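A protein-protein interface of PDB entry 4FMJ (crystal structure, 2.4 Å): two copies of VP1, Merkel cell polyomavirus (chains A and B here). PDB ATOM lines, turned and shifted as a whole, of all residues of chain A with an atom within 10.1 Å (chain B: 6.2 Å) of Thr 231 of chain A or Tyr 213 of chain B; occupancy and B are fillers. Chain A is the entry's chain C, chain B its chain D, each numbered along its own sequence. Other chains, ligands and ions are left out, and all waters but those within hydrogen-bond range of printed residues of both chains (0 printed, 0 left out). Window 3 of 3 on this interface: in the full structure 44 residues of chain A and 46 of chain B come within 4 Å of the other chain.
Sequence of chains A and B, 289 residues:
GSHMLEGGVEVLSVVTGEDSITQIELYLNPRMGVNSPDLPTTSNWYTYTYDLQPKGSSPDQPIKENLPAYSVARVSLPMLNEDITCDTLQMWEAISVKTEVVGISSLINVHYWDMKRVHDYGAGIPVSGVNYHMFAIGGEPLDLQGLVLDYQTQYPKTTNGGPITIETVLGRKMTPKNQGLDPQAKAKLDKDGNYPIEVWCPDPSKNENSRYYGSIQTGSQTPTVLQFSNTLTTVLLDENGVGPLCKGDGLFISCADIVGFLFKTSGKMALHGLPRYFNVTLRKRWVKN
Positions printed for both chains: 97, 234 and 235.
Of the 11 pairs that touch across the chains among the printed residues, none has its exchanged pair printed and touching as well.
OE2 of Glu 100 of chain A sits at hydrogen-bond distance from OH of Tyr 212 of chain B, 2.7 Å away.
The backbone carbonyl oxygen of Phe 228 of chain A lies within hydrogen-bond range of the backbone NH of Gly 214 of chain B (2.8 Å).
The side-chain hydroxyl (OG) of Ser 229 of chain A is in hydrogen-bond range of the backbone carbonyl oxygen (O) of Tyr 212 of chain B (2.7 Å).
OD1 of Asn 230 of chain A lies within hydrogen-bond range of N of Tyr 212 of chain B, at 3.0 Å.
Printed residues of chain A that touch a printed residue of chain B: Glu 100, Leu 226, Gln 227, Phe 228, Ser 229, Asn 230 and Thr 231.
Hydrophobic or aromatic side chains of chain A within 4 Å of the printed part of chain B: Phe 228.
Of the 15 printed residues of chain B, 5 touch a printed residue of chain A.
Hydrophobic or aromatic side chains of chain B within 4 Å of the printed part of chain A: Tyr 212 and Tyr 213.
Among the printed residues, 11 pairs touch across the chains.
O of Asn 230 of chain A sits at hydrogen-bond distance from NZ of Lys 98 of chain A (2.7 Å).
The side-chain carboxylate (OE1) of Glu 100 of chain A lies close to the backbone NH (N) of Ser 229 of chain A, 3.4 Å away.
O of Glu 100 of chain A is in hydrogen-bond range of N of Tyr 277 of chain A (2.9 Å).
The backbone NH of Ser 215 of chain B is in hydrogen-bond range of the backbone carbonyl oxygen of His 133 of chain B (2.8 Å).
O of Ile 137 of chain B sits at hydrogen-bond distance from N of Arg 211 of chain B.
NE of Arg 211 of chain B is in hydrogen-bond range of O of Leu 236 of chain B, 2.8 Å away.
Printed residues of chain B within 4 Å of Glu 100 of chain A: Tyr 212 (2.7 Å).
Of the printed residues of chain B, Gln 227 of chain A touches Gly 214 (3.3 Å).
Printed residues of chain B within 4 Å of Thr 231 of chain A: Tyr 213.
No residue of chain A comes within 4 Å of Met 134 of chain B.
No residue of chain A comes within 4 Å of Phe 135 of chain B.
Ala 136 of chain B touches none of the printed residues of chain A.
Of the printed residues of chain A, Tyr 213 of chain B touches Phe 228 (3.6 Å), Ser 229 (3.4 Å) and Thr 231 (3.5 Å).
Gly 214 of chain B touches just these residues of chain A: Gln 227 and Phe 228.
The nearest residue of chain B that does not touch Thr 231 of chain A is Arg 211 of chain B (4.3 Å).
The nearest printed residue of chain B that does not touch Gln 227 of chain A is Ser 215 of chain B (4.2 Å).
CA of Ser 215 of chain B touches O of Leu 226 of chain A, at 3.1 Å.
Gln 227 of chain A touches Gly 214 of chain B.
O of Phe 228 of chain A touches C of Tyr 213 of chain B, 3.6 Å away.
Phe 228 of chain A touches Ser 215 of chain B (CE1 to N, 3.4 Å).
OG of Ser 229 of chain A touches CD1 of Tyr 213 of chain B, at 3.4 Å.
Arg 211 of chain B touches Asn 230 of chain A.
Thr 231 of chain A touches Tyr 213 of chain B.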
ATOM      1  N   VAL A  97     -16.046 -36.510 -20.086  1.00  0.00           N
ATOM      2  CA  VAL A  97     -14.946 -36.373 -21.035  1.00  0.00           C
ATOM      3  C   VAL A  97     -14.026 -35.199 -20.669  1.00  0.00           C
ATOM      4  O   VAL A  97     -14.494 -34.141 -20.247  1.00  0.00           O
ATOM      5  CB  VAL A  97     -15.460 -36.256 -22.514  1.00  0.00           C
ATOM      6  CG1 VAL A  97     -16.204 -34.936 -22.759  1.00  0.00           C
ATOM      7  CG2 VAL A  97     -14.320 -36.418 -23.508  1.00  0.00           C
ATOM      8  N   LYS A  98     -12.719 -35.422 -20.794  1.00  0.00           N
ATOM      9  CA  LYS A  98     -11.733 -34.340 -20.823  1.00  0.00           C
ATOM     10  C   LYS A  98     -11.266 -34.209 -22.265  1.00  0.00           C
ATOM     11  O   LYS A  98     -10.847 -35.194 -22.876  1.00  0.00           O
ATOM     12  CB  LYS A  98     -10.521 -34.649 -19.942  1.00  0.00           C
ATOM     13  CG  LYS A  98     -10.791 -34.781 -18.458  1.00  0.00           C
ATOM     14  CD  LYS A  98      -9.505 -34.558 -17.673  1.00  0.00           C
ATOM     15  CE  LYS A  98      -9.741 -34.767 -16.198  1.00  0.00           C
ATOM     16  NZ  LYS A  98      -8.666 -34.190 -15.346  1.00  0.00           N
ATOM     17  N   THR A  99     -11.338 -32.998 -22.805  1.00  0.00           N
ATOM     18  CA  THR A  99     -10.980 -32.743 -24.196  1.00  0.00           C
ATOM     19  C   THR A  99     -10.169 -31.455 -24.318  1.00  0.00           C
ATOM     20  O   THR A  99     -10.237 -30.582 -23.457  1.00  0.00           O
ATOM     21  CB  THR A  99     -12.236 -32.719 -25.109  1.00  0.00           C
ATOM     22  OG1 THR A  99     -11.848 -32.694 -26.486  1.00  0.00           O
ATOM     23  CG2 THR A  99     -13.128 -31.519 -24.797  1.00  0.00           C
ATOM     24  N   GLU A 100      -9.391 -31.334 -25.385  1.00  0.00           N
ATOM     25  CA  GLU A 100      -8.432 -30.233 -25.482  1.00  0.00           C
ATOM     26  C   GLU A 100      -7.906 -30.092 -26.895  1.00  0.00           C
ATOM     27  O   GLU A 100      -7.606 -31.084 -27.561  1.00  0.00           O
ATOM     28  CB  GLU A 100      -7.278 -30.476 -24.509  1.00  0.00           C
ATOM     29  CG  GLU A 100      -6.225 -29.395 -24.453  1.00  0.00           C
ATOM     30  CD  GLU A 100      -5.359 -29.510 -23.209  1.00  0.00           C
ATOM     31  OE1 GLU A 100      -5.927 -29.560 -22.090  1.00  0.00           O
ATOM     32  OE2 GLU A 100      -4.113 -29.549 -23.355  1.00  0.00           O
ATOM     33  N   ILE A 104      -1.851 -25.260 -29.516  1.00  0.00           N
ATOM     34  CA  ILE A 104      -2.290 -23.872 -29.460  1.00  0.00           C
ATOM     35  C   ILE A 104      -1.076 -22.948 -29.454  1.00  0.00           C
ATOM     36  O   ILE A 104      -1.046 -21.937 -30.163  1.00  0.00           O
ATOM     37  CB  ILE A 104      -3.204 -23.615 -28.233  1.00  0.00           C
ATOM     38  CG1 ILE A 104      -4.599 -24.174 -28.501  1.00  0.00           C
ATOM     39  CG2 ILE A 104      -3.301 -22.130 -27.903  1.00  0.00           C
ATOM     40  CD1 ILE A 104      -5.315 -24.688 -27.259  1.00  0.00           C
ATOM     41  N   LEU A 226      -8.187 -18.939 -27.333  1.00  0.00           N
ATOM     42  CA  LEU A 226      -8.430 -20.316 -26.900  1.00  0.00           C
ATOM     43  C   LEU A 226      -7.816 -20.595 -25.548  1.00  0.00           C
ATOM     44  O   LEU A 226      -6.807 -19.992 -25.187  1.00  0.00           O
ATOM     45  CB  LEU A 226      -7.888 -21.325 -27.929  1.00  0.00           C
ATOM     46  CG  LEU A 226      -8.246 -21.130 -29.408  1.00  0.00           C
ATOM     47  CD1 LEU A 226      -7.454 -22.087 -30.313  1.00  0.00           C
ATOM     48  CD2 LEU A 226      -9.741 -21.283 -29.646  1.00  0.00           C
ATOM     49  N   GLN A 227      -8.436 -21.515 -24.809  1.00  0.00           N
ATOM     50  CA  GLN A 227      -7.961 -21.920 -23.490  1.00  0.00           C
ATOM     51  C   GLN A 227      -7.558 -23.382 -23.510  1.00  0.00           C
ATOM     52  O   GLN A 227      -8.048 -24.158 -24.336  1.00  0.00           O
ATOM     53  CB  GLN A 227      -9.047 -21.722 -22.422  1.00  0.00           C
ATOM     54  CG  GLN A 227      -9.476 -20.269 -22.170  1.00  0.00           C
ATOM     55  CD  GLN A 227     -10.455 -19.759 -23.221  1.00  0.00           C
ATOM     56  OE1 GLN A 227     -11.363 -20.482 -23.641  1.00  0.00           O
ATOM     57  NE2 GLN A 227     -10.277 -18.509 -23.649  1.00  0.00           N
ATOM     58  N   PHE A 228      -6.667 -23.753 -22.588  1.00  0.00           N
ATOM     59  CA  PHE A 228      -6.278 -25.147 -22.392  1.00  0.00           C
ATOM     60  C   PHE A 228      -5.993 -25.438 -20.929  1.00  0.00           C
ATOM     61  O   PHE A 228      -5.372 -24.632 -20.231  1.00  0.00           O
ATOM     62  CB  PHE A 228      -5.102 -25.559 -23.304  1.00  0.00           C
ATOM     63  CG  PHE A 228      -3.902 -24.642 -23.234  1.00  0.00           C
ATOM     64  CD1 PHE A 228      -3.863 -23.448 -23.974  1.00  0.00           C
ATOM     65  CD2 PHE A 228      -2.802 -24.977 -22.453  1.00  0.00           C
ATOM     66  CE1 PHE A 228      -2.757 -22.600 -23.925  1.00  0.00           C
ATOM     67  CE2 PHE A 228      -1.686 -24.135 -22.396  1.00  0.00           C
ATOM     68  CZ  PHE A 228      -1.661 -22.943 -23.140  1.00  0.00           C
ATOM     69  N   SER A 229      -6.475 -26.590 -20.466  1.00  0.00           N
ATOM     70  CA  SER A 229      -6.275 -27.035 -19.082  1.00  0.00           C
ATOM     71  C   SER A 229      -6.610 -28.522 -18.922  1.00  0.00           C
ATOM     72  O   SER A 229      -7.565 -29.009 -19.526  1.00  0.00           O
ATOM     73  CB  SER A 229      -7.133 -26.202 -18.123  1.00  0.00           C
ATOM     74  OG  SER A 229      -6.728 -26.400 -16.785  1.00  0.00           O
ATOM     75  N   ASN A 230      -5.833 -29.239 -18.107  1.00  0.00           N
ATOM     76  CA  ASN A 230      -6.171 -30.629 -17.779  1.00  0.00           C
ATOM     77  C   ASN A 230      -7.098 -30.793 -16.571  1.00  0.00           C
ATOM     78  O   ASN A 230      -7.341 -31.925 -16.144  1.00  0.00           O
ATOM     79  CB  ASN A 230      -4.916 -31.503 -17.625  1.00  0.00           C
ATOM     80  CG  ASN A 230      -4.039 -31.090 -16.460  1.00  0.00           C
ATOM     81  OD1 ASN A 230      -4.157 -29.978 -15.915  1.00  0.00           O
ATOM     82  ND2 ASN A 230      -3.148 -31.994 -16.060  1.00  0.00           N
ATOM     83  N   THR A 231      -7.607 -29.670 -16.037  1.00  0.00           N
ATOM     84  CA  THR A 231      -8.593 -29.668 -14.942  1.00  0.00           C
ATOM     85  C   THR A 231     -10.058 -29.578 -15.421  1.00  0.00           C
ATOM     86  O   THR A 231     -10.982 -29.756 -14.632  1.00  0.00           O
ATOM     87  CB  THR A 231      -8.337 -28.509 -13.916  1.00  0.00           C
ATOM     88  OG1 THR A 231      -8.638 -27.249 -14.521  1.00  0.00           O
ATOM     89  CG2 THR A 231      -6.885 -28.487 -13.436  1.00  0.00           C
ATOM     90  N   LEU A 232     -10.279 -29.291 -16.698  1.00  0.00           N
ATOM     91  CA  LEU A 232     -11.640 -29.116 -17.215  1.00  0.00           C
ATOM     92  C   LEU A 232     -12.294 -30.449 -17.592  1.00  0.00           C
ATOM     93  O   LEU A 232     -11.688 -31.255 -18.294  1.00  0.00           O
ATOM     94  CB  LEU A 232     -11.641 -28.204 -18.451  1.00  0.00           C
ATOM     95  CG  LEU A 232     -11.138 -26.757 -18.411  1.00  0.00           C
ATOM     96  CD1 LEU A 232     -11.221 -26.141 -19.816  1.00  0.00           C
ATOM     97  CD2 LEU A 232     -11.878 -25.883 -17.378  1.00  0.00           C
ATOM     98  N   THR A 233     -13.534 -30.653 -17.151  1.00  0.00           N
ATOM     99  CA  THR A 233     -14.301 -31.870 -17.450  1.00  0.00           C
ATOM    100  C   THR A 233     -15.724 -31.536 -17.899  1.00  0.00           C
ATOM    101  O   THR A 233     -16.402 -30.729 -17.267  1.00  0.00           O
ATOM    102  CB  THR A 233     -14.364 -32.813 -16.220  1.00  0.00           C
ATOM    103  OG1 THR A 233     -13.034 -33.070 -15.747  1.00  0.00           O
ATOM    104  CG2 THR A 233     -15.031 -34.146 -16.572  1.00  0.00           C
ATOM    105  N   THR A 234     -16.167 -32.157 -18.990  1.00  0.00           N
ATOM    106  CA  THR A 234     -17.562 -32.063 -19.434  1.00  0.00           C
ATOM    107  C   THR A 234     -18.340 -33.313 -19.000  1.00  0.00           C
ATOM    108  O   THR A 234     -17.939 -34.444 -19.302  1.00  0.00           O
ATOM    109  CB  THR A 234     -17.668 -31.907 -20.968  1.00  0.00           C
ATOM    110  OG1 THR A 234     -16.752 -30.901 -21.412  1.00  0.00           O
ATOM    111  CG2 THR A 234     -19.076 -31.517 -21.388  1.00  0.00           C
ATOM    112  N   VAL A 235     -19.447 -33.087 -18.294  1.00  0.00           N
ATOM    113  CA  VAL A 235     -20.351 -34.150 -17.835  1.00  0.00           C
ATOM    114  C   VAL A 235     -21.321 -34.469 -18.967  1.00  0.00           C
ATOM    115  O   VAL A 235     -21.930 -33.557 -19.530  1.00  0.00           O
ATOM    116  CB  VAL A 235     -21.123 -33.702 -16.568  1.00  0.00           C
ATOM    117  CG1 VAL A 235     -22.250 -34.661 -16.238  1.00  0.00           C
ATOM    118  CG2 VAL A 235     -20.173 -33.559 -15.381  1.00  0.00           C
ATOM    119  N   TYR A 277      -7.575 -33.842 -28.549  1.00  0.00           N
ATOM    120  CA  TYR A 277      -7.400 -35.027 -27.706  1.00  0.00           C
ATOM    121  C   TYR A 277      -8.636 -35.284 -26.831  1.00  0.00           C
ATOM    122  O   TYR A 277      -9.290 -34.344 -26.388  1.00  0.00           O
ATOM    123  CB  TYR A 277      -6.145 -34.862 -26.842  1.00  0.00           C
ATOM    124  CG  TYR A 277      -6.063 -35.787 -25.650  1.00  0.00           C
ATOM    125  CD1 TYR A 277      -5.512 -37.059 -25.766  1.00  0.00           C
ATOM    126  CD2 TYR A 277      -6.538 -35.390 -24.406  1.00  0.00           C
ATOM    127  CE1 TYR A 277      -5.440 -37.912 -24.664  1.00  0.00           C
ATOM    128  CE2 TYR A 277      -6.473 -36.235 -23.302  1.00  0.00           C
ATOM    129  CZ  TYR A 277      -5.918 -37.491 -23.432  1.00  0.00           C
ATOM    130  OH  TYR A 277      -5.845 -38.325 -22.331  1.00  0.00           O
ATOM    131  N   VAL B  97      -2.534 -22.942  -4.887  1.00  0.00           N
ATOM    132  CA  VAL B  97      -1.542 -21.976  -5.348  1.00  0.00           C
ATOM    133  C   VAL B  97      -2.121 -20.577  -5.526  1.00  0.00           C
ATOM    134  O   VAL B  97      -3.243 -20.410  -6.013  1.00  0.00           O
ATOM    135  CB  VAL B  97      -0.834 -22.449  -6.647  1.00  0.00           C
ATOM    136  CG1 VAL B  97      -1.830 -22.671  -7.766  1.00  0.00           C
ATOM    137  CG2 VAL B  97       0.285 -21.462  -7.068  1.00  0.00           C
ATOM    138  N   HIS B 133      -0.397 -17.017 -22.112  1.00  0.00           N
ATOM    139  CA  HIS B 133      -0.259 -17.177 -20.669  1.00  0.00           C
ATOM    140  C   HIS B 133      -0.525 -18.597 -20.239  1.00  0.00           C
ATOM    141  O   HIS B 133      -1.462 -19.231 -20.744  1.00  0.00           O
ATOM    142  CB  HIS B 133      -1.154 -16.186 -19.926  1.00  0.00           C
ATOM    143  CG  HIS B 133      -0.856 -14.764 -20.269  1.00  0.00           C
ATOM    144  ND1 HIS B 133       0.054 -14.007 -19.566  1.00  0.00           N
ATOM    145  CD2 HIS B 133      -1.295 -13.982 -21.282  1.00  0.00           C
ATOM    146  CE1 HIS B 133       0.138 -12.806 -20.111  1.00  0.00           C
ATOM    147  NE2 HIS B 133      -0.667 -12.766 -21.157  1.00  0.00           N
ATOM    148  N   MET B 134       0.332 -19.097 -19.341  1.00  0.00           N
ATOM    149  CA  MET B 134       0.231 -20.461 -18.813  1.00  0.00           C
ATOM    150  C   MET B 134       1.089 -20.668 -17.575  1.00  0.00           C
ATOM    151  O   MET B 134       2.174 -20.101 -17.444  1.00  0.00           O
ATOM    152  CB  MET B 134       0.570 -21.511 -19.893  1.00  0.00           C
ATOM    153  CG  MET B 134       2.048 -21.897 -20.022  1.00  0.00           C
ATOM    154  SD  MET B 134       2.540 -23.256 -18.913  1.00  0.00           S
ATOM    155  CE  MET B 134       1.786 -24.664 -19.714  1.00  0.00           C
ATOM    156  N   PHE B 135       0.594 -21.488 -16.662  1.00  0.00           N
ATOM    157  CA  PHE B 135       1.388 -21.914 -15.533  1.00  0.00           C
ATOM    158  C   PHE B 135       1.006 -23.341 -15.190  1.00  0.00           C
ATOM    159  O   PHE B 135      -0.095 -23.788 -15.524  1.00  0.00           O
ATOM    160  CB  PHE B 135       1.196 -20.978 -14.331  1.00  0.00           C
ATOM    161  CG  PHE B 135      -0.164 -21.089 -13.653  1.00  0.00           C
ATOM    162  CD1 PHE B 135      -1.225 -20.267 -14.042  1.00  0.00           C
ATOM    163  CD2 PHE B 135      -0.367 -21.990 -12.607  1.00  0.00           C
ATOM    164  CE1 PHE B 135      -2.479 -20.345 -13.409  1.00  0.00           C
ATOM    165  CE2 PHE B 135      -1.614 -22.081 -11.959  1.00  0.00           C
ATOM    166  CZ  PHE B 135      -2.675 -21.255 -12.363  1.00  0.00           C
ATOM    167  N   ALA B 136       1.922 -24.043 -14.522  1.00  0.00           N
ATOM    168  CA  ALA B 136       1.729 -25.427 -14.133  1.00  0.00           C
ATOM    169  C   ALA B 136       2.401 -25.708 -12.799  1.00  0.00           C
ATOM    170  O   ALA B 136       3.487 -25.188 -12.526  1.00  0.00           O
ATOM    171  CB  ALA B 136       2.266 -26.369 -15.212  1.00  0.00           C
ATOM    172  N   ILE B 137       1.723 -26.507 -11.968  1.00  0.00           N
ATOM    173  CA  ILE B 137       2.278 -27.072 -10.734  1.00  0.00           C
ATOM    174  C   ILE B 137       2.206 -28.599 -10.843  1.00  0.00           C
ATOM    175  O   ILE B 137       1.159 -29.156 -11.200  1.00  0.00           O
ATOM    176  CB  ILE B 137       1.511 -26.616  -9.458  1.00  0.00           C
ATOM    177  CG1 ILE B 137       1.171 -25.113  -9.492  1.00  0.00           C
ATOM    178  CG2 ILE B 137       2.307 -26.979  -8.201  1.00  0.00           C
ATOM    179  CD1 ILE B 137       2.378 -24.160  -9.450  1.00  0.00           C
ATOM    180  N   ARG B 211      -0.894 -30.149 -12.717  1.00  0.00           N
ATOM    181  CA  ARG B 211      -2.027 -29.300 -13.090  1.00  0.00           C
ATOM    182  C   ARG B 211      -1.512 -28.132 -13.945  1.00  0.00           C
ATOM    183  O   ARG B 211      -0.513 -27.488 -13.590  1.00  0.00           O
ATOM    184  CB  ARG B 211      -2.714 -28.756 -11.828  1.00  0.00           C
ATOM    185  CG  ARG B 211      -3.044 -29.801 -10.745  1.00  0.00           C
ATOM    186  CD  ARG B 211      -4.052 -30.860 -11.228  1.00  0.00           C
ATOM    187  NE  ARG B 211      -4.361 -31.815 -10.164  1.00  0.00           N
ATOM    188  CZ  ARG B 211      -3.870 -33.049 -10.072  1.00  0.00           C
ATOM    189  NH1 ARG B 211      -3.042 -33.538 -10.997  1.00  0.00           N
ATOM    190  NH2 ARG B 211      -4.225 -33.805  -9.045  1.00  0.00           N
ATOM    191  N   TYR B 212      -2.179 -27.855 -15.062  1.00  0.00           N
ATOM    192  CA  TYR B 212      -1.770 -26.737 -15.929  1.00  0.00           C
ATOM    193  C   TYR B 212      -2.960 -25.908 -16.428  1.00  0.00           C
ATOM    194  O   TYR B 212      -4.096 -26.382 -16.442  1.00  0.00           O
ATOM    195  CB  TYR B 212      -0.841 -27.202 -17.071  1.00  0.00           C
ATOM    196  CG  TYR B 212      -1.456 -28.119 -18.120  1.00  0.00           C
ATOM    197  CD1 TYR B 212      -2.247 -27.606 -19.146  1.00  0.00           C
ATOM    198  CD2 TYR B 212      -1.208 -29.489 -18.112  1.00  0.00           C
ATOM    199  CE1 TYR B 212      -2.802 -28.438 -20.121  1.00  0.00           C
ATOM    200  CE2 TYR B 212      -1.754 -30.333 -19.089  1.00  0.00           C
ATOM    201  CZ  TYR B 212      -2.555 -29.794 -20.088  1.00  0.00           C
ATOM    202  OH  TYR B 212      -3.110 -30.598 -21.059  1.00  0.00           O
ATOM    203  N   TYR B 213      -2.695 -24.654 -16.788  1.00  0.00           N
ATOM    204  CA  TYR B 213      -3.742 -23.710 -17.162  1.00  0.00           C
ATOM    205  C   TYR B 213      -3.138 -22.737 -18.163  1.00  0.00           C
ATOM    206  O   TYR B 213      -2.112 -22.116 -17.884  1.00  0.00           O
ATOM    207  CB  TYR B 213      -4.257 -22.923 -15.925  1.00  0.00           C
ATOM    208  CG  TYR B 213      -4.549 -23.773 -14.706  1.00  0.00           C
ATOM    209  CD1 TYR B 213      -5.854 -24.177 -14.396  1.00  0.00           C
ATOM    210  CD2 TYR B 213      -3.510 -24.197 -13.872  1.00  0.00           C
ATOM    211  CE1 TYR B 213      -6.108 -24.977 -13.272  1.00  0.00           C
ATOM    212  CE2 TYR B 213      -3.747 -24.995 -12.770  1.00  0.00           C
ATOM    213  CZ  TYR B 213      -5.037 -25.383 -12.470  1.00  0.00           C
ATOM    214  OH  TYR B 213      -5.227 -26.175 -11.364  1.00  0.00           O
ATOM    215  N   GLY B 214      -3.771 -22.580 -19.316  1.00  0.00           N
ATOM    216  CA  GLY B 214      -3.265 -21.641 -20.299  1.00  0.00           C
ATOM    217  C   GLY B 214      -4.277 -21.054 -21.262  1.00  0.00           C
ATOM    218  O   GLY B 214      -5.406 -21.545 -21.364  1.00  0.00           O
ATOM    219  N   SER B 215      -3.853 -19.999 -21.965  1.00  0.00           N
ATOM    220  CA  SER B 215      -4.649 -19.348 -23.008  1.00  0.00           C
ATOM    221  C   SER B 215      -3.750 -18.596 -23.991  1.00  0.00           C
ATOM    222  O   SER B 215      -2.573 -18.334 -23.706  1.00  0.00           O
ATOM    223  CB  SER B 215      -5.683 -18.389 -22.396  1.00  0.00           C
ATOM    224  OG  SER B 215      -5.048 -17.297 -21.754  1.00  0.00           O
ATOM    225  N   THR B 234      -5.984 -20.850  -6.623  1.00  0.00           N
ATOM    226  CA  THR B 234      -6.327 -22.022  -7.436  1.00  0.00           C
ATOM    227  C   THR B 234      -6.236 -23.283  -6.552  1.00  0.00           C
ATOM    228  O   THR B 234      -5.228 -23.504  -5.873  1.00  0.00           O
ATOM    229  CB  THR B 234      -5.409 -22.128  -8.674  1.00  0.00           C
ATOM    230  OG1 THR B 234      -5.565 -20.956  -9.480  1.00  0.00           O
ATOM    231  CG2 THR B 234      -5.726 -23.369  -9.529  1.00  0.00           C
ATOM    232  N   VAL B 235      -7.308 -24.080  -6.546  1.00  0.00           N
ATOM    233  CA  VAL B 235      -7.328 -25.378  -5.860  1.00  0.00           C
ATOM    234  C   VAL B 235      -6.730 -26.435  -6.807  1.00  0.00           C
ATOM    235  O   VAL B 235      -7.165 -26.562  -7.951  1.00  0.00           O
ATOM    236  CB  VAL B 235      -8.776 -25.761  -5.382  1.00  0.00           C
ATOM    237  CG1 VAL B 235      -8.908 -27.260  -5.118  1.00  0.00           C
ATOM    238  CG2 VAL B 235      -9.170 -24.963  -4.121  1.00  0.00           C
ATOM    239  N   LEU B 236      -5.736 -27.179  -6.326  1.00  0.00           N
ATOM    240  CA  LEU B 236      -4.964 -28.096  -7.174  1.00  0.00           C
ATOM    241  C   LEU B 236      -5.415 -29.553  -7.073  1.00  0.00           C
ATOM    242  O   LEU B 236      -4.948 -30.404  -7.837  1.00  0.00           O
ATOM    243  CB  LEU B 236      -3.464 -28.000  -6.853  1.00  0.00           C
ATOM    244  CG  LEU B 236      -2.746 -26.661  -7.076  1.00  0.00           C
ATOM    245  CD1 LEU B 236      -1.395 -26.627  -6.356  1.00  0.00           C
ATOM    246  CD2 LEU B 236      -2.594 -26.351  -8.567  1.00  0.00           C
ATOM    247  N   GLU B 239     -10.509 -34.581  -8.830  1.00  0.00           N
ATOM    248  CA  GLU B 239     -11.885 -34.956  -8.459  1.00  0.00           C
ATOM    249  C   GLU B 239     -11.965 -35.953  -7.307  1.00  0.00           C
ATOM    250  O   GLU B 239     -13.001 -36.052  -6.659  1.00  0.00           O
ATOM    251  CB  GLU B 239     -12.697 -35.462  -9.669  1.00  0.00           C
ATOM    252  CG  GLU B 239     -12.111 -36.666 -10.422  1.00  0.00           C
ATOM    253  CD  GLU B 239     -10.946 -36.290 -11.350  1.00  0.00           C
ATOM    254  OE1 GLU B 239     -10.690 -35.070 -11.544  1.00  0.00           O
ATOM    255  OE2 GLU B 239     -10.286 -37.219 -11.885  1.00  0.00           O
